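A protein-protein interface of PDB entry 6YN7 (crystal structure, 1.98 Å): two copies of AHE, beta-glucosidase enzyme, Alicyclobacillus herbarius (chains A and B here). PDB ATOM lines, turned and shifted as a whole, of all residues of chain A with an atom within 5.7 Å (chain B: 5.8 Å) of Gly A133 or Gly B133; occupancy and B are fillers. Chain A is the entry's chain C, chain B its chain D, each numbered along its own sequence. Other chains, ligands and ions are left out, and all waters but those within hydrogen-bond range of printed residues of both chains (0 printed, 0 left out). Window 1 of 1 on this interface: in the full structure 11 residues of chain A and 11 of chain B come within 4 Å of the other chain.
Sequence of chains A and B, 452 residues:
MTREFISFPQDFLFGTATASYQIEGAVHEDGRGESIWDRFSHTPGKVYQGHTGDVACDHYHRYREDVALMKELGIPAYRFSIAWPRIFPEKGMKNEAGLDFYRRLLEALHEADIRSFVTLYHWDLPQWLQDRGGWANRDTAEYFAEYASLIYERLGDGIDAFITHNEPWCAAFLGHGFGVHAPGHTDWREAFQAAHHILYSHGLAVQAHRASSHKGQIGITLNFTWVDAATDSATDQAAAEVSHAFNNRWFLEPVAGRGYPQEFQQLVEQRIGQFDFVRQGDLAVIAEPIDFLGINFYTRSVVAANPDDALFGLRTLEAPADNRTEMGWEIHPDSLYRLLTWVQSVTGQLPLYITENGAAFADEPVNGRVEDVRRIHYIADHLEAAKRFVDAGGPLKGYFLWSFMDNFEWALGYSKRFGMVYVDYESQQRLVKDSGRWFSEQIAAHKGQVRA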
ATOM      1  N   LEU A 129     -10.084  -0.946   4.216  1.00  0.00           N
ATOM      2  CA  LEU A 129      -9.382  -2.055   4.851  1.00  0.00           C
ATOM      3  C   LEU A 129      -8.814  -3.010   3.808  1.00  0.00           C
ATOM      4  O   LEU A 129      -7.738  -3.586   4.005  1.00  0.00           O
ATOM      5  CB  LEU A 129     -10.319  -2.794   5.805  1.00  0.00           C
ATOM      6  CG  LEU A 129     -10.468  -2.168   7.192  1.00  0.00           C
ATOM      7  CD1 LEU A 129     -11.653  -2.771   7.925  1.00  0.00           C
ATOM      8  CD2 LEU A 129      -9.188  -2.345   7.994  1.00  0.00           C
ATOM      9  N   GLN A 130      -9.524  -3.192   2.692  1.00  0.00           N
ATOM     10  CA  GLN A 130      -8.990  -4.007   1.606  1.00  0.00           C
ATOM     11  C   GLN A 130      -7.773  -3.345   0.975  1.00  0.00           C
ATOM     12  O   GLN A 130      -6.826  -4.031   0.570  1.00  0.00           O
ATOM     13  CB  GLN A 130     -10.072  -4.259   0.556  1.00  0.00           C
ATOM     14  CG  GLN A 130      -9.618  -5.112  -0.615  1.00  0.00           C
ATOM     15  CD  GLN A 130      -9.205  -6.505  -0.191  1.00  0.00           C
ATOM     16  OE1 GLN A 130      -9.842  -7.123   0.662  1.00  0.00           O
ATOM     17  NE2 GLN A 130      -8.129  -7.011  -0.785  1.00  0.00           N
ATOM     18  N   ASP A 131      -7.780  -2.012   0.883  1.00  0.00           N
ATOM     19  CA  ASP A 131      -6.609  -1.295   0.391  1.00  0.00           C
ATOM     20  C   ASP A 131      -5.401  -1.535   1.287  1.00  0.00           C
ATOM     21  O   ASP A 131      -4.257  -1.451   0.825  1.00  0.00           O
ATOM     22  CB  ASP A 131      -6.912   0.201   0.287  1.00  0.00           C
ATOM     23  CG  ASP A 131      -7.611   0.572  -1.013  1.00  0.00           C
ATOM     24  OD1 ASP A 131      -8.106  -0.337  -1.713  1.00  0.00           O
ATOM     25  OD2 ASP A 131      -7.661   1.777  -1.338  1.00  0.00           O
ATOM     26  N   ARG A 132      -5.633  -1.842   2.566  1.00  0.00           N
ATOM     27  CA  ARG A 132      -4.574  -2.193   3.503  1.00  0.00           C
ATOM     28  C   ARG A 132      -4.360  -3.699   3.602  1.00  0.00           C
ATOM     29  O   ARG A 132      -3.874  -4.189   4.631  1.00  0.00           O
ATOM     30  CB  ARG A 132      -4.876  -1.607   4.883  1.00  0.00           C
ATOM     31  CG  ARG A 132      -5.177  -0.118   4.870  1.00  0.00           C
ATOM     32  CD  ARG A 132      -5.035   0.481   6.258  1.00  0.00           C
ATOM     33  NE  ARG A 132      -3.719   0.212   6.827  1.00  0.00           N
ATOM     34  CZ  ARG A 132      -3.053   1.062   7.604  1.00  0.00           C
ATOM     35  NH1 ARG A 132      -3.583   2.238   7.908  1.00  0.00           N
ATOM     36  NH2 ARG A 132      -1.858   0.735   8.076  1.00  0.00           N
ATOM     37  N   GLY A 133      -4.719  -4.449   2.561  1.00  0.00           N
ATOM     38  CA  GLY A 133      -4.516  -5.880   2.533  1.00  0.00           C
ATOM     39  C   GLY A 133      -5.707  -6.707   2.969  1.00  0.00           C
ATOM     40  O   GLY A 133      -5.783  -7.890   2.617  1.00  0.00           O
ATOM     41  N   GLY A 134      -6.632  -6.125   3.729  1.00  0.00           N
ATOM     42  CA  GLY A 134      -7.818  -6.861   4.130  1.00  0.00           C
ATOM     43  C   GLY A 134      -7.486  -7.999   5.077  1.00  0.00           C
ATOM     44  O   GLY A 134      -6.698  -7.853   6.018  1.00  0.00           O
ATOM     45  N   TRP A 135      -8.092  -9.159   4.817  1.00  0.00           N
ATOM     46  CA  TRP A 135      -7.952 -10.307   5.704  1.00  0.00           C
ATOM     47  C   TRP A 135      -6.595 -10.989   5.596  1.00  0.00           C
ATOM     48  O   TRP A 135      -6.270 -11.818   6.453  1.00  0.00           O
ATOM     49  CB  TRP A 135      -9.075 -11.310   5.435  1.00  0.00           C
ATOM     50  CG  TRP A 135     -10.385 -10.853   6.000  1.00  0.00           C
ATOM     51  CD1 TRP A 135     -11.521 -10.557   5.307  1.00  0.00           C
ATOM     52  CD2 TRP A 135     -10.684 -10.616   7.381  1.00  0.00           C
ATOM     53  NE1 TRP A 135     -12.513 -10.159   6.170  1.00  0.00           N
ATOM     54  CE2 TRP A 135     -12.024 -10.188   7.450  1.00  0.00           C
ATOM     55  CE3 TRP A 135      -9.950 -10.731   8.566  1.00  0.00           C
ATOM     56  CZ2 TRP A 135     -12.646  -9.873   8.657  1.00  0.00           C
ATOM     57  CZ3 TRP A 135     -10.568 -10.417   9.760  1.00  0.00           C
ATOM     58  CH2 TRP A 135     -11.902  -9.993   9.797  1.00  0.00           C
ATOM     59  N   ALA A 136      -5.798 -10.668   4.576  1.00  0.00           N
ATOM     60  CA  ALA A 136      -4.407 -11.099   4.574  1.00  0.00           C
ATOM     61  C   ALA A 136      -3.589 -10.357   5.620  1.00  0.00           C
ATOM     62  O   ALA A 136      -2.547 -10.862   6.052  1.00  0.00           O
ATOM     63  CB  ALA A 136      -3.791 -10.904   3.188  1.00  0.00           C
ATOM     64  N   ASN A 137      -4.044  -9.177   6.035  1.00  0.00           N
ATOM     65  CA  ASN A 137      -3.377  -8.389   7.061  1.00  0.00           C
ATOM     66  C   ASN A 137      -3.974  -8.716   8.425  1.00  0.00           C
ATOM     67  O   ASN A 137      -5.197  -8.691   8.597  1.00  0.00           O
ATOM     68  CB  ASN A 137      -3.516  -6.896   6.764  1.00  0.00           C
ATOM     69  CG  ASN A 137      -2.639  -6.038   7.652  1.00  0.00           C
ATOM     70  OD1 ASN A 137      -1.810  -6.549   8.405  1.00  0.00           O
ATOM     71  ND2 ASN A 137      -2.811  -4.724   7.564  1.00  0.00           N
ATOM     72  N   THR A 140      -6.494  -6.316  10.381  1.00  0.00           N
ATOM     73  CA  THR A 140      -7.929  -6.348  10.114  1.00  0.00           C
ATOM     74  C   THR A 140      -8.678  -7.084  11.217  1.00  0.00           C
ATOM     75  O   THR A 140      -9.779  -6.677  11.609  1.00  0.00           O
ATOM     76  CB  THR A 140      -8.197  -7.004   8.760  1.00  0.00           C
ATOM     77  OG1 THR A 140      -7.523  -6.269   7.730  1.00  0.00           O
ATOM     78  CG2 THR A 140      -9.688  -7.034   8.460  1.00  0.00           C
ATOM     79  N   GLU A 190      -2.715 -16.842   0.436  1.00  0.00           N
ATOM     80  CA  GLU A 190      -3.475 -15.707   0.946  1.00  0.00           C
ATOM     81  C   GLU A 190      -4.833 -16.142   1.479  1.00  0.00           C
ATOM     82  O   GLU A 190      -5.328 -15.571   2.457  1.00  0.00           O
ATOM     83  CB  GLU A 190      -3.638 -14.662  -0.160  1.00  0.00           C
ATOM     84  CG  GLU A 190      -4.549 -13.497   0.187  1.00  0.00           C
ATOM     85  CD  GLU A 190      -4.773 -12.566  -0.990  1.00  0.00           C
ATOM     86  OE1 GLU A 190      -4.281 -12.873  -2.097  1.00  0.00           O
ATOM     87  OE2 GLU A 190      -5.441 -11.526  -0.810  1.00  0.00           O
ATOM     88  N   LEU B 129       4.898  -6.666   2.714  1.00  0.00           N
ATOM     89  CA  LEU B 129       4.324  -5.383   2.322  1.00  0.00           C
ATOM     90  C   LEU B 129       3.081  -5.583   1.466  1.00  0.00           C
ATOM     91  O   LEU B 129       2.127  -4.800   1.553  1.00  0.00           O
ATOM     92  CB  LEU B 129       5.362  -4.547   1.577  1.00  0.00           C
ATOM     93  CG  LEU B 129       6.263  -3.668   2.440  1.00  0.00           C
ATOM     94  CD1 LEU B 129       7.336  -3.028   1.586  1.00  0.00           C
ATOM     95  CD2 LEU B 129       5.438  -2.609   3.155  1.00  0.00           C
ATOM     96  N   GLN B 130       3.074  -6.624   0.631  1.00  0.00           N
ATOM     97  CA  GLN B 130       1.883  -6.932  -0.153  1.00  0.00           C
ATOM     98  C   GLN B 130       0.740  -7.403   0.734  1.00  0.00           C
ATOM     99  O   GLN B 130      -0.428  -7.120   0.442  1.00  0.00           O
ATOM    100  CB  GLN B 130       2.208  -7.987  -1.211  1.00  0.00           C
ATOM    101  CG  GLN B 130       1.064  -8.282  -2.162  1.00  0.00           C
ATOM    102  CD  GLN B 130       0.581  -7.044  -2.886  1.00  0.00           C
ATOM    103  OE1 GLN B 130       1.369  -6.158  -3.221  1.00  0.00           O
ATOM    104  NE2 GLN B 130      -0.723  -6.970  -3.128  1.00  0.00           N
ATOM    105  N   ASP B 131       1.053  -8.119   1.817  1.00  0.00           N
ATOM    106  CA  ASP B 131       0.026  -8.503   2.778  1.00  0.00           C
ATOM    107  C   ASP B 131      -0.610  -7.291   3.441  1.00  0.00           C
ATOM    108  O   ASP B 131      -1.721  -7.398   3.975  1.00  0.00           O
ATOM    109  CB  ASP B 131       0.616  -9.436   3.838  1.00  0.00           C
ATOM    110  CG  ASP B 131       0.852 -10.841   3.314  1.00  0.00           C
ATOM    111  OD1 ASP B 131       0.572 -11.087   2.121  1.00  0.00           O
ATOM    112  OD2 ASP B 131       1.312 -11.700   4.094  1.00  0.00           O
ATOM    113  N   ARG B 132       0.065  -6.142   3.419  1.00  0.00           N
ATOM    114  CA  ARG B 132      -0.487  -4.887   3.906  1.00  0.00           C
ATOM    115  C   ARG B 132      -1.123  -4.061   2.795  1.00  0.00           C
ATOM    116  O   ARG B 132      -1.338  -2.857   2.975  1.00  0.00           O
ATOM    117  CB  ARG B 132       0.598  -4.070   4.608  1.00  0.00           C
ATOM    118  CG  ARG B 132       1.413  -4.855   5.620  1.00  0.00           C
ATOM    119  CD  ARG B 132       1.725  -4.005   6.834  1.00  0.00           C
ATOM    120  NE  ARG B 132       0.502  -3.501   7.452  1.00  0.00           N
ATOM    121  CZ  ARG B 132       0.465  -2.818   8.591  1.00  0.00           C
ATOM    122  NH1 ARG B 132       1.588  -2.550   9.243  1.00  0.00           N
ATOM    123  NH2 ARG B 132      -0.696  -2.401   9.079  1.00  0.00           N
ATOM    124  N   GLY B 133      -1.422  -4.673   1.651  1.00  0.00           N
ATOM    125  CA  GLY B 133      -2.045  -3.981   0.545  1.00  0.00           C
ATOM    126  C   GLY B 133      -1.091  -3.509  -0.530  1.00  0.00           C
ATOM    127  O   GLY B 133      -1.552  -3.091  -1.601  1.00  0.00           O
ATOM    128  N   GLY B 134       0.215  -3.559  -0.280  1.00  0.00           N
ATOM    129  CA  GLY B 134       1.176  -3.184  -1.301  1.00  0.00           C
ATOM    130  C   GLY B 134       1.048  -1.727  -1.690  1.00  0.00           C
ATOM    131  O   GLY B 134       0.839  -0.846  -0.848  1.00  0.00           O
ATOM    132  N   TRP B 135       1.163  -1.467  -2.990  1.00  0.00           N
ATOM    133  CA  TRP B 135       1.123  -0.104  -3.501  1.00  0.00           C
ATOM    134  C   TRP B 135      -0.278   0.493  -3.505  1.00  0.00           C
ATOM    135  O   TRP B 135      -0.416   1.703  -3.708  1.00  0.00           O
ATOM    136  CB  TRP B 135       1.721  -0.061  -4.908  1.00  0.00           C
ATOM    137  CG  TRP B 135       3.199  -0.288  -4.906  1.00  0.00           C
ATOM    138  CD1 TRP B 135       3.862  -1.393  -5.354  1.00  0.00           C
ATOM    139  CD2 TRP B 135       4.201   0.609  -4.411  1.00  0.00           C
ATOM    140  NE1 TRP B 135       5.217  -1.235  -5.177  1.00  0.00           N
ATOM    141  CE2 TRP B 135       5.450  -0.014  -4.600  1.00  0.00           C
ATOM    142  CE3 TRP B 135       4.163   1.881  -3.832  1.00  0.00           C
ATOM    143  CZ2 TRP B 135       6.650   0.592  -4.229  1.00  0.00           C
ATOM    144  CZ3 TRP B 135       5.352   2.479  -3.466  1.00  0.00           C
ATOM    145  CH2 TRP B 135       6.578   1.836  -3.665  1.00  0.00           C
ATOM    146  N   ALA B 136      -1.317  -0.317  -3.291  1.00  0.00           N
ATOM    147  CA  ALA B 136      -2.636   0.245  -3.038  1.00  0.00           C
ATOM    148  C   ALA B 136      -2.697   0.938  -1.686  1.00  0.00           C
ATOM    149  O   ALA B 136      -3.568   1.788  -1.474  1.00  0.00           O
ATOM    150  CB  ALA B 136      -3.705  -0.846  -3.118  1.00  0.00           C
ATOM    151  N   ASN B 137      -1.788   0.594  -0.778  1.00  0.00           N
ATOM    152  CA  ASN B 137      -1.694   1.214   0.535  1.00  0.00           C
ATOM    153  C   ASN B 137      -0.648   2.320   0.492  1.00  0.00           C
ATOM    154  O   ASN B 137       0.474   2.100   0.022  1.00  0.00           O
ATOM    155  CB  ASN B 137      -1.332   0.175   1.599  1.00  0.00           C
ATOM    156  CG  ASN B 137      -1.327   0.748   3.004  1.00  0.00           C
ATOM    157  OD1 ASN B 137      -1.657   1.916   3.216  1.00  0.00           O
ATOM    158  ND2 ASN B 137      -0.960  -0.079   3.976  1.00  0.00           N
ATOM    159  N   THR B 140       3.049   2.007   2.035  1.00  0.00           N
ATOM    160  CA  THR B 140       4.150   1.438   1.266  1.00  0.00           C
ATOM    161  C   THR B 140       5.063   2.522   0.709  1.00  0.00           C
ATOM    162  O   THR B 140       6.280   2.323   0.616  1.00  0.00           O
ATOM    163  CB  THR B 140       3.602   0.573   0.130  1.00  0.00           C
ATOM    164  OG1 THR B 140       2.706  -0.408   0.667  1.00  0.00           O
ATOM    165  CG2 THR B 140       4.732  -0.133  -0.611  1.00  0.00           C
ATOM    166  N   HIS B 176      -1.362  -4.554 -11.237  1.00  0.00           N
ATOM    167  CA  HIS B 176      -2.647  -4.341 -10.586  1.00  0.00           C
ATOM    168  C   HIS B 176      -3.808  -4.129 -11.546  1.00  0.00           C
ATOM    169  O   HIS B 176      -4.961  -4.213 -11.108  1.00  0.00           O
ATOM    170  CB  HIS B 176      -2.571  -3.142  -9.628  1.00  0.00           C
ATOM    171  CG  HIS B 176      -1.387  -3.172  -8.711  1.00  0.00           C
ATOM    172  ND1 HIS B 176      -0.125  -2.786  -9.108  1.00  0.00           N
ATOM    173  CD2 HIS B 176      -1.275  -3.545  -7.414  1.00  0.00           C
ATOM    174  CE1 HIS B 176       0.714  -2.921  -8.096  1.00  0.00           C
ATOM    175  NE2 HIS B 176       0.041  -3.379  -7.056  1.00  0.00           N
ATOM    176  N   GLU B 190      -7.512   0.160  -8.388  1.00  0.00           N
ATOM    177  CA  GLU B 190      -6.333  -0.175  -7.599  1.00  0.00           C
ATOM    178  C   GLU B 190      -5.049   0.123  -8.361  1.00  0.00           C
ATOM    179  O   GLU B 190      -4.035   0.485  -7.753  1.00  0.00           O
ATOM    180  CB  GLU B 190      -6.390  -1.649  -7.195  1.00  0.00           C
ATOM    181  CG  GLU B 190      -5.180  -2.151  -6.428  1.00  0.00           C
ATOM    182  CD  GLU B 190      -5.239  -3.644  -6.169  1.00  0.00           C
ATOM    183  OE1 GLU B 190      -6.262  -4.271  -6.525  1.00  0.00           O
ATOM    184  OE2 GLU B 190      -4.268  -4.193  -5.609  1.00  0.00           O
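Of the 11 printed residues of chain A, 5 touch a printed residue of chain B.
Printed residues of chain A that touch a printed residue of chain B: Asp A131, Arg A132, Gly A133, Ala A136 and Asn A137.
Among the printed residues, 14 pairs touch across the chains.
Arg B132 touches Asp A131.
Asp A131 touches Ala B136 (O to C, 3.8 Å).
CB of Asn B137 touches O of Asp A131, 3.4 Å away.
Asp B131 touches Arg A132 (O to O, 3.9 Å).
N of Gly B133 touches C of Arg A132, at 3.7 Å.
Asn B137 touches Arg A132 (ND2 to NE, 3.98 Å).
Gly A133 touches Asp B131.
Arg B132 touches Gly A133.
Asp B131 touches Ala A136 (O to C, 3.9 Å).
CB of Asn A137 touches O of Asp B131 (3.4 Å).
Of the printed residues of chain B, Asp A131 touches Arg B132 (3.9 Å), Gly B133 (3.4 Å), Ala B136 (3.8 Å) and Asn B137 (3.4 Å).
Printed residues of chain B within 4 Å of Arg A132: Asp B131 (3.9 Å), Arg B132 (3.2 Å), Gly B133 (3.7 Å) and Asn B137 (3.98 Å).
Gly A133 touches just these residues of chain B: Asp B131, Arg B132 and Gly B133.
Gly A134 touches none of the printed residues of chain B.
Of the printed residues of chain B, Ala A136 touches Asp B131 (3.9 Å).
Of chain A, only Asp A131 (3.4 Å), Arg A132 (3.7 Å) and Gly A133 (3.4 Å) come within 4 Å of Gly B133.
Printed residues of chain A within 4 Å of Ala B136: Asp A131 (3.8 Å).
The backbone carbonyl oxygen (O) of Asn A137 sits close to the side-chain hydroxyl (OG1) of Thr A140, at 3.5 Å.
O of Asn B137 is in hydrogen-bond range of OG1 of Thr B140 (3.4 Å).
The backbone carbonyl oxygen (O) of Arg B132 is in hydrogen-bond range of the side-chain amide nitrogen (ND2) of Asn B137, 3.0 Å away.
O of Arg A132 sits at hydrogen-bond distance from ND2 of Asn A137 (3.2 Å).
Asp A131 touches Arg B132, and with the chains exchanged Arg A132 touches Asp B131.
Asp A131 touches Gly B133, and with the chains exchanged Gly A133 touches Asp B131.
Arg A132 touches its own counterpart, Arg B132.
Gly B133 touches its own counterpart, Gly A133.
Positions printed for both chains: 129, 130, 131, 132, 133, 134, 135, 136, 137, 140 and 190.
Of the 14 pairs that touch across the chains among the printed residues, 14 have their exchanged pair printed and touching as well.
The side-chain amide nitrogen of Asn A137 sits close to the guanidinium group of Arg B132 (3.5 Å).
The backbone carbonyl oxygen (O) of Arg B132 sits close to the backbone carbonyl oxygen (O) of Arg A132, at 3.3 Å.
The backbone NH (N) of Gly A133 lies close to the backbone NH (N) of Gly B133, at 3.4 Å.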
